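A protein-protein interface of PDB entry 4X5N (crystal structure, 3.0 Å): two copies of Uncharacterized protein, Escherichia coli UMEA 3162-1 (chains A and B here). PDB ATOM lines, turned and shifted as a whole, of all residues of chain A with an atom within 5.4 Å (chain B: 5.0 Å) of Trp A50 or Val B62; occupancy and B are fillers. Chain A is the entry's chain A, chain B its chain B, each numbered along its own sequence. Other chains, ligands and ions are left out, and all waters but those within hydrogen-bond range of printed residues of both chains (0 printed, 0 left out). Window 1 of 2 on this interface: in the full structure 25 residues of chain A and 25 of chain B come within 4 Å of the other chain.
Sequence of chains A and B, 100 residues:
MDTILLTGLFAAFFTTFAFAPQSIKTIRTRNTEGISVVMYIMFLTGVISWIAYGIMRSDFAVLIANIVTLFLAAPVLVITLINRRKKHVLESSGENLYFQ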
ATOM      1  N   THR A  45      -0.146  28.529   4.680  1.00  0.00           N
ATOM      2  CA  THR A  45      -0.396  27.095   4.795  1.00  0.00           C
ATOM      3  C   THR A  45      -0.963  26.545   3.490  1.00  0.00           C
ATOM      4  O   THR A  45      -0.566  25.470   3.037  1.00  0.00           O
ATOM      5  CB  THR A  45      -1.366  26.761   5.946  1.00  0.00           C
ATOM      6  OG1 THR A  45      -1.641  27.944   6.703  1.00  0.00           O
ATOM      7  CG2 THR A  45      -0.765  25.708   6.859  1.00  0.00           C
ATOM      8  N   GLY A  46      -1.894  27.284   2.893  1.00  0.00           N
ATOM      9  CA  GLY A  46      -2.466  26.895   1.619  1.00  0.00           C
ATOM     10  C   GLY A  46      -1.447  26.985   0.501  1.00  0.00           C
ATOM     11  O   GLY A  46      -1.443  26.161  -0.417  1.00  0.00           O
ATOM     12  N   VAL A  47      -0.575  27.987   0.588  1.00  0.00           N
ATOM     13  CA  VAL A  47       0.454  28.205  -0.422  1.00  0.00           C
ATOM     14  C   VAL A  47       1.378  26.996  -0.537  1.00  0.00           C
ATOM     15  O   VAL A  47       1.590  26.473  -1.631  1.00  0.00           O
ATOM     16  CB  VAL A  47       1.285  29.467  -0.112  1.00  0.00           C
ATOM     17  CG1 VAL A  47       2.515  29.532  -1.001  1.00  0.00           C
ATOM     18  CG2 VAL A  47       0.434  30.718  -0.289  1.00  0.00           C
ATOM     19  N   ILE A  48       1.907  26.548   0.597  1.00  0.00           N
ATOM     20  CA  ILE A  48       2.775  25.375   0.633  1.00  0.00           C
ATOM     21  C   ILE A  48       2.012  24.130   0.189  1.00  0.00           C
ATOM     22  O   ILE A  48       2.566  23.250  -0.470  1.00  0.00           O
ATOM     23  CB  ILE A  48       3.363  25.157   2.038  1.00  0.00           C
ATOM     24  CG1 ILE A  48       4.176  26.381   2.465  1.00  0.00           C
ATOM     25  CG2 ILE A  48       4.221  23.900   2.078  1.00  0.00           C
ATOM     26  CD1 ILE A  48       5.044  26.152   3.688  1.00  0.00           C
ATOM     27  N   SER A  49       0.733  24.069   0.545  1.00  0.00           N
ATOM     28  CA  SER A  49      -0.127  22.978   0.108  1.00  0.00           C
ATOM     29  C   SER A  49      -0.300  23.016  -1.409  1.00  0.00           C
ATOM     30  O   SER A  49      -0.325  21.975  -2.063  1.00  0.00           O
ATOM     31  CB  SER A  49      -1.484  23.055   0.808  1.00  0.00           C
ATOM     32  OG  SER A  49      -1.326  23.308   2.192  1.00  0.00           O
ATOM     33  N   TRP A  50      -0.416  24.223  -1.958  1.00  0.00           N
ATOM     34  CA  TRP A  50      -0.500  24.410  -3.404  1.00  0.00           C
ATOM     35  C   TRP A  50       0.799  24.002  -4.092  1.00  0.00           C
ATOM     36  O   TRP A  50       0.788  23.462  -5.200  1.00  0.00           O
ATOM     37  CB  TRP A  50      -0.825  25.864  -3.746  1.00  0.00           C
ATOM     38  CG  TRP A  50      -2.287  26.198  -3.725  1.00  0.00           C
ATOM     39  CD1 TRP A  50      -2.923  27.044  -2.864  1.00  0.00           C
ATOM     40  CD2 TRP A  50      -3.293  25.699  -4.612  1.00  0.00           C
ATOM     41  NE1 TRP A  50      -4.263  27.100  -3.158  1.00  0.00           N
ATOM     42  CE2 TRP A  50      -4.517  26.282  -4.228  1.00  0.00           C
ATOM     43  CE3 TRP A  50      -3.279  24.814  -5.695  1.00  0.00           C
ATOM     44  CZ2 TRP A  50      -5.715  26.008  -4.889  1.00  0.00           C
ATOM     45  CZ3 TRP A  50      -4.470  24.541  -6.349  1.00  0.00           C
ATOM     46  CH2 TRP A  50      -5.670  25.137  -5.945  1.00  0.00           C
ATOM     47  N   ILE A  51       1.918  24.287  -3.436  1.00  0.00           N
ATOM     48  CA  ILE A  51       3.222  23.874  -3.933  1.00  0.00           C
ATOM     49  C   ILE A  51       3.273  22.353  -4.040  1.00  0.00           C
ATOM     50  O   ILE A  51       3.776  21.805  -5.020  1.00  0.00           O
ATOM     51  CB  ILE A  51       4.360  24.383  -3.017  1.00  0.00           C
ATOM     52  CG1 ILE A  51       4.466  25.909  -3.100  1.00  0.00           C
ATOM     53  CG2 ILE A  51       5.691  23.733  -3.381  1.00  0.00           C
ATOM     54  CD1 ILE A  51       5.573  26.492  -2.248  1.00  0.00           C
ATOM     55  N   ALA A  52       2.728  21.682  -3.030  1.00  0.00           N
ATOM     56  CA  ALA A  52       2.656  20.227  -3.017  1.00  0.00           C
ATOM     57  C   ALA A  52       1.728  19.716  -4.111  1.00  0.00           C
ATOM     58  O   ALA A  52       1.957  18.657  -4.690  1.00  0.00           O
ATOM     59  CB  ALA A  52       2.189  19.738  -1.662  1.00  0.00           C
ATOM     60  N   TYR A  53       0.678  20.479  -4.389  1.00  0.00           N
ATOM     61  CA  TYR A  53      -0.288  20.103  -5.409  1.00  0.00           C
ATOM     62  C   TYR A  53       0.322  20.227  -6.805  1.00  0.00           C
ATOM     63  O   TYR A  53       0.091  19.377  -7.671  1.00  0.00           O
ATOM     64  CB  TYR A  53      -1.548  20.963  -5.290  1.00  0.00           C
ATOM     65  CG  TYR A  53      -2.676  20.525  -6.192  1.00  0.00           C
ATOM     66  CD1 TYR A  53      -3.435  19.404  -5.891  1.00  0.00           C
ATOM     67  CD2 TYR A  53      -2.984  21.234  -7.346  1.00  0.00           C
ATOM     68  CE1 TYR A  53      -4.466  19.001  -6.710  1.00  0.00           C
ATOM     69  CE2 TYR A  53      -4.014  20.837  -8.174  1.00  0.00           C
ATOM     70  CZ  TYR A  53      -4.751  19.719  -7.851  1.00  0.00           C
ATOM     71  OH  TYR A  53      -5.776  19.325  -8.678  1.00  0.00           O
ATOM     72  N   GLY A  54       1.105  21.283  -7.018  1.00  0.00           N
ATOM     73  CA  GLY A  54       1.772  21.497  -8.290  1.00  0.00           C
ATOM     74  C   GLY A  54       2.744  20.380  -8.619  1.00  0.00           C
ATOM     75  O   GLY A  54       2.863  19.965  -9.772  1.00  0.00           O
ATOM     76  N   ILE A  55       3.440  19.895  -7.596  1.00  0.00           N
ATOM     77  CA  ILE A  55       4.334  18.752  -7.730  1.00  0.00           C
ATOM     78  C   ILE A  55       3.543  17.488  -8.045  1.00  0.00           C
ATOM     79  O   ILE A  55       3.929  16.697  -8.908  1.00  0.00           O
ATOM     80  CB  ILE A  55       5.157  18.530  -6.443  1.00  0.00           C
ATOM     81  CG1 ILE A  55       5.984  19.774  -6.119  1.00  0.00           C
ATOM     82  CG2 ILE A  55       6.051  17.303  -6.575  1.00  0.00           C
ATOM     83  CD1 ILE A  55       6.807  19.647  -4.857  1.00  0.00           C
ATOM     84  N   VAL A  62       0.819  26.531 -11.742  1.00  0.00           N
ATOM     85  CA  VAL A  62       0.318  26.725 -10.383  1.00  0.00           C
ATOM     86  C   VAL A  62       1.443  26.594  -9.351  1.00  0.00           C
ATOM     87  O   VAL A  62       1.343  27.124  -8.244  1.00  0.00           O
ATOM     88  CB  VAL A  62      -0.810  25.719 -10.048  1.00  0.00           C
ATOM     89  CG1 VAL A  62      -0.235  24.339  -9.781  1.00  0.00           C
ATOM     90  CG2 VAL A  62      -1.623  26.196  -8.851  1.00  0.00           C
ATOM     91  N   LEU A  63       2.519  25.904  -9.717  1.00  0.00           N
ATOM     92  CA  LEU A  63       3.632  25.695  -8.795  1.00  0.00           C
ATOM     93  C   LEU A  63       4.428  26.984  -8.595  1.00  0.00           C
ATOM     94  O   LEU A  63       4.506  27.502  -7.483  1.00  0.00           O
ATOM     95  CB  LEU A  63       4.551  24.577  -9.297  1.00  0.00           C
ATOM     96  CG  LEU A  63       5.789  24.284  -8.443  1.00  0.00           C
ATOM     97  CD1 LEU A  63       5.399  23.997  -7.004  1.00  0.00           C
ATOM     98  CD2 LEU A  63       6.587  23.122  -9.023  1.00  0.00           C
ATOM     99  N   ASN A  66       2.701  29.867  -6.860  1.00  0.00           N
ATOM    100  CA  ASN A  66       2.681  29.801  -5.409  1.00  0.00           C
ATOM    101  C   ASN A  66       4.088  29.806  -4.815  1.00  0.00           C
ATOM    102  O   ASN A  66       4.259  30.049  -3.622  1.00  0.00           O
ATOM    103  CB  ASN A  66       1.917  28.564  -4.946  1.00  0.00           C
ATOM    104  CG  ASN A  66       0.450  28.606  -5.336  1.00  0.00           C
ATOM    105  OD1 ASN A  66      -0.362  29.246  -4.669  1.00  0.00           O
ATOM    106  ND2 ASN A  66       0.105  27.921  -6.420  1.00  0.00           N
ATOM    107  N   GLY B   8      -5.328  19.260  -2.811  1.00  0.00           N
ATOM    108  CA  GLY B   8      -5.667  20.470  -3.540  1.00  0.00           C
ATOM    109  C   GLY B   8      -6.832  21.243  -2.948  1.00  0.00           C
ATOM    110  O   GLY B   8      -6.801  22.473  -2.895  1.00  0.00           O
ATOM    111  N   ALA B  11      -5.555  22.961  -0.024  1.00  0.00           N
ATOM    112  CA  ALA B  11      -4.840  24.127  -0.521  1.00  0.00           C
ATOM    113  C   ALA B  11      -5.833  25.189  -0.972  1.00  0.00           C
ATOM    114  O   ALA B  11      -5.648  26.374  -0.698  1.00  0.00           O
ATOM    115  CB  ALA B  11      -3.919  23.742  -1.660  1.00  0.00           C
ATOM    116  N   ALA B  12      -6.886  24.759  -1.661  1.00  0.00           N
ATOM    117  CA  ALA B  12      -7.905  25.680  -2.154  1.00  0.00           C
ATOM    118  C   ALA B  12      -8.560  26.449  -1.015  1.00  0.00           C
ATOM    119  O   ALA B  12      -8.562  27.679  -1.013  1.00  0.00           O
ATOM    120  CB  ALA B  12      -8.957  24.929  -2.954  1.00  0.00           C
ATOM    121  N   THR B  15      -6.329  29.144   0.813  1.00  0.00           N
ATOM    122  CA  THR B  15      -5.887  30.301   0.035  1.00  0.00           C
ATOM    123  C   THR B  15      -6.988  31.336  -0.168  1.00  0.00           C
ATOM    124  O   THR B  15      -6.745  32.537  -0.036  1.00  0.00           O
ATOM    125  CB  THR B  15      -5.353  29.886  -1.348  1.00  0.00           C
ATOM    126  OG1 THR B  15      -5.428  28.462  -1.489  1.00  0.00           O
ATOM    127  CG2 THR B  15      -3.913  30.340  -1.512  1.00  0.00           C
ATOM    128  N   TRP B  50      -7.515  31.928 -14.911  1.00  0.00           N
ATOM    129  CA  TRP B  50      -7.351  30.711 -14.122  1.00  0.00           C
ATOM    130  C   TRP B  50      -8.517  29.755 -14.341  1.00  0.00           C
ATOM    131  O   TRP B  50      -8.328  28.541 -14.423  1.00  0.00           O
ATOM    132  CB  TRP B  50      -7.221  31.040 -12.633  1.00  0.00           C
ATOM    133  CG  TRP B  50      -5.814  31.329 -12.191  1.00  0.00           C
ATOM    134  CD1 TRP B  50      -5.328  32.513 -11.718  1.00  0.00           C
ATOM    135  CD2 TRP B  50      -4.712  30.413 -12.181  1.00  0.00           C
ATOM    136  NE1 TRP B  50      -3.994  32.392 -11.415  1.00  0.00           N
ATOM    137  CE2 TRP B  50      -3.591  31.111 -11.691  1.00  0.00           C
ATOM    138  CE3 TRP B  50      -4.564  29.070 -12.541  1.00  0.00           C
ATOM    139  CZ2 TRP B  50      -2.339  30.511 -11.551  1.00  0.00           C
ATOM    140  CZ3 TRP B  50      -3.321  28.475 -12.402  1.00  0.00           C
ATOM    141  CH2 TRP B  50      -2.226  29.195 -11.911  1.00  0.00           C
ATOM    142  N   TYR B  53      -7.955  28.175 -17.554  1.00  0.00           N
ATOM    143  CA  TYR B  53      -6.863  27.219 -17.425  1.00  0.00           C
ATOM    144  C   TYR B  53      -7.340  25.936 -16.751  1.00  0.00           C
ATOM    145  O   TYR B  53      -6.871  24.843 -17.073  1.00  0.00           O
ATOM    146  CB  TYR B  53      -5.707  27.836 -16.639  1.00  0.00           C
ATOM    147  CG  TYR B  53      -4.514  26.922 -16.477  1.00  0.00           C
ATOM    148  CD1 TYR B  53      -3.681  26.637 -17.551  1.00  0.00           C
ATOM    149  CD2 TYR B  53      -4.215  26.353 -15.247  1.00  0.00           C
ATOM    150  CE1 TYR B  53      -2.586  25.808 -17.406  1.00  0.00           C
ATOM    151  CE2 TYR B  53      -3.124  25.522 -15.092  1.00  0.00           C
ATOM    152  CZ  TYR B  53      -2.312  25.254 -16.175  1.00  0.00           C
ATOM    153  OH  TYR B  53      -1.222  24.427 -16.029  1.00  0.00           O
ATOM    154  N   GLY B  54      -8.277  26.077 -15.817  1.00  0.00           N
ATOM    155  CA  GLY B  54      -8.842  24.933 -15.126  1.00  0.00           C
ATOM    156  C   GLY B  54      -9.680  24.057 -16.037  1.00  0.00           C
ATOM    157  O   GLY B  54      -9.631  22.831 -15.944  1.00  0.00           O
ATOM    158  N   ASP B  59      -8.887  20.513 -13.999  1.00  0.00           N
ATOM    159  CA  ASP B  59      -8.461  20.608 -12.606  1.00  0.00           C
ATOM    160  C   ASP B  59      -9.563  21.267 -11.772  1.00  0.00           C
ATOM    161  O   ASP B  59      -9.806  22.467 -11.891  1.00  0.00           O
ATOM    162  CB  ASP B  59      -7.147  21.393 -12.509  1.00  0.00           C
ATOM    163  CG  ASP B  59      -6.522  21.337 -11.123  1.00  0.00           C
ATOM    164  OD1 ASP B  59      -7.206  21.670 -10.133  1.00  0.00           O
ATOM    165  OD2 ASP B  59      -5.333  20.968 -11.027  1.00  0.00           O
ATOM    166  N   PHE B  60     -10.223  20.476 -10.929  1.00  0.00           N
ATOM    167  CA  PHE B  60     -11.357  20.959 -10.146  1.00  0.00           C
ATOM    168  C   PHE B  60     -10.932  22.021  -9.139  1.00  0.00           C
ATOM    169  O   PHE B  60     -11.573  23.065  -9.017  1.00  0.00           O
ATOM    170  CB  PHE B  60     -12.037  19.794  -9.423  1.00  0.00           C
ATOM    171  CG  PHE B  60     -13.306  20.174  -8.721  1.00  0.00           C
ATOM    172  CD1 PHE B  60     -14.449  20.477  -9.446  1.00  0.00           C
ATOM    173  CD2 PHE B  60     -13.362  20.217  -7.337  1.00  0.00           C
ATOM    174  CE1 PHE B  60     -15.623  20.824  -8.803  1.00  0.00           C
ATOM    175  CE2 PHE B  60     -14.534  20.562  -6.687  1.00  0.00           C
ATOM    176  CZ  PHE B  60     -15.665  20.865  -7.423  1.00  0.00           C
ATOM    177  N   ALA B  61      -9.838  21.746  -8.436  1.00  0.00           N
ATOM    178  CA  ALA B  61      -9.337  22.612  -7.371  1.00  0.00           C
ATOM    179  C   ALA B  61      -9.057  24.044  -7.826  1.00  0.00           C
ATOM    180  O   ALA B  61      -9.498  24.997  -7.184  1.00  0.00           O
ATOM    181  CB  ALA B  61      -8.080  22.008  -6.767  1.00  0.00           C
ATOM    182  N   VAL B  62      -8.316  24.198  -8.920  1.00  0.00           N
ATOM    183  CA  VAL B  62      -7.972  25.528  -9.412  1.00  0.00           C
ATOM    184  C   VAL B  62      -9.192  26.207 -10.032  1.00  0.00           C
ATOM    185  O   VAL B  62      -9.243  27.431 -10.137  1.00  0.00           O
ATOM    186  CB  VAL B  62      -6.823  25.484 -10.447  1.00  0.00           C
ATOM    187  CG1 VAL B  62      -5.633  24.707  -9.894  1.00  0.00           C
ATOM    188  CG2 VAL B  62      -7.298  24.880 -11.755  1.00  0.00           C
ATOM    189  N   LEU B  63     -10.177  25.405 -10.432  1.00  0.00           N
ATOM    190  CA  LEU B  63     -11.419  25.931 -10.991  1.00  0.00           C
ATOM    191  C   LEU B  63     -12.311  26.487  -9.888  1.00  0.00           C
ATOM    192  O   LEU B  63     -12.664  27.665  -9.905  1.00  0.00           O
ATOM    193  CB  LEU B  63     -12.167  24.850 -11.781  1.00  0.00           C
ATOM    194  CG  LEU B  63     -13.459  25.298 -12.473  1.00  0.00           C
ATOM    195  CD1 LEU B  63     -13.167  26.329 -13.551  1.00  0.00           C
ATOM    196  CD2 LEU B  63     -14.211  24.110 -13.057  1.00  0.00           C
ATOM    197  N   ILE B  64     -12.660  25.636  -8.927  1.00  0.00           N
ATOM    198  CA  ILE B  64     -13.554  26.020  -7.838  1.00  0.00           C
ATOM    199  C   ILE B  64     -12.977  27.161  -6.997  1.00  0.00           C
ATOM    200  O   ILE B  64     -13.715  28.023  -6.517  1.00  0.00           O
ATOM    201  CB  ILE B  64     -13.872  24.807  -6.919  1.00  0.00           C
ATOM    202  CG1 ILE B  64     -14.878  25.191  -5.834  1.00  0.00           C
ATOM    203  CG2 ILE B  64     -12.599  24.229  -6.301  1.00  0.00           C
ATOM    204  CD1 ILE B  64     -15.123  24.099  -4.812  1.00  0.00           C
ATOM    205  N   ALA B  65     -11.656  27.180  -6.841  1.00  0.00           N
ATOM    206  CA  ALA B  65     -11.008  28.183  -6.004  1.00  0.00           C
ATOM    207  C   ALA B  65     -11.174  29.581  -6.583  1.00  0.00           C
ATOM    208  O   ALA B  65     -11.644  30.492  -5.901  1.00  0.00           O
ATOM    209  CB  ALA B  65      -9.531  27.859  -5.826  1.00  0.00           C
ATOM    210  N   ASN B  66     -10.789  29.745  -7.845  1.00  0.00           N
ATOM    211  CA  ASN B  66     -10.835  31.050  -8.489  1.00  0.00           C
ATOM    212  C   ASN B  66     -12.247  31.480  -8.882  1.00  0.00           C
ATOM    213  O   ASN B  66     -12.501  32.668  -9.061  1.00  0.00           O
ATOM    214  CB  ASN B  66      -9.929  31.066  -9.718  1.00  0.00           C
ATOM    215  CG  ASN B  66      -8.489  31.413  -9.377  1.00  0.00           C
ATOM    216  OD1 ASN B  66      -7.639  30.533  -9.239  1.00  0.00           O
ATOM    217  ND2 ASN B  66      -8.211  32.704  -9.241  1.00  0.00           N
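Trp A50 touches just these residues of chain B: Ala B11, Ala B12, Thr B15 and Val B62.
Val B62 touches just one residue of chain A: Trp A50 (3.7 Å).
Printed residues of chain A within 4 Å of Trp B50: Val A62.
Printed residues of chain A within 4 Å of Ala B12: Trp A50.
Printed residues of chain B within 4 Å of Tyr A53: Gly B8 (3.4 Å) and Asp B59 (2.9 Å).
Of the printed residues of chain B, Gly A46 touches Ala B11 (3.7 Å).
Asn B66 touches none of the printed residues of chain A.
The nearest residue of chain B that does not touch Trp A50 is Ala B61 (4.03 Å).
The nearest residue of chain A that does not touch Val B62 is Val A62 (4.4 Å).
Printed residues of chain B that touch a printed residue of chain A: Gly B8, Ala B11, Ala B12, Thr B15, Trp B50, Asp B59 and Val B62.
Hydrophobic or aromatic side chains of chain B that line the printed part of chain A: Ala B11, Ala B12, Trp B50 and Val B62.
Hydrophobic or aromatic side chains of chain A within 4 Å of the printed part of chain B: Trp A50 and Tyr A53.
Among the printed residues, no Asp or Glu carboxylate lies within 4 Å of a Lys or Arg side-chain nitrogen of the other chain.
Gly A46 touches Ala B11.
Ser A49 touches Ala B11 (CB to CB, 3.5 Å).
Trp A50 touches Ala B12 (CZ2 to CA, 3.5 Å).
Val B62 touches Trp A50 (CG1 to CZ3, 3.7 Å).
Gly B8 touches Tyr A53.
Val A62 touches Trp B50.
Trp A50 touches Val B62, and with the chains exchanged Val A62 touches Trp B50.
6 positions are printed for both chains.
O of Ala B11 is in hydrogen-bond range of NE1 of Trp A50 (2.9 Å).
OG1 of Thr B15 is in hydrogen-bond range of NE1 of Trp A50, at 2.4 Å.
The side-chain hydroxyl of Tyr A53 sits at hydrogen-bond distance from the side-chain carboxylate of Asp B59.
O of Thr A45 lies within hydrogen-bond range of OG of Ser A49 (2.4 Å).
The backbone carbonyl oxygen (O) of Ala B12 lies within hydrogen-bond range of the side-chain hydroxyl (OG1) of Thr B15 (3.3 Å).
The backbone NH of Asp B59 sits at hydrogen-bond distance from the backbone carbonyl oxygen of Gly B54 (3.1 Å).
The side-chain carboxylate of Asp B59 sits at hydrogen-bond distance from the backbone NH of Ala B61.
The side-chain carboxylate (OD1) of Asp B59 sits at hydrogen-bond distance from the backbone NH (N) of Val B62, at 3.0 Å.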
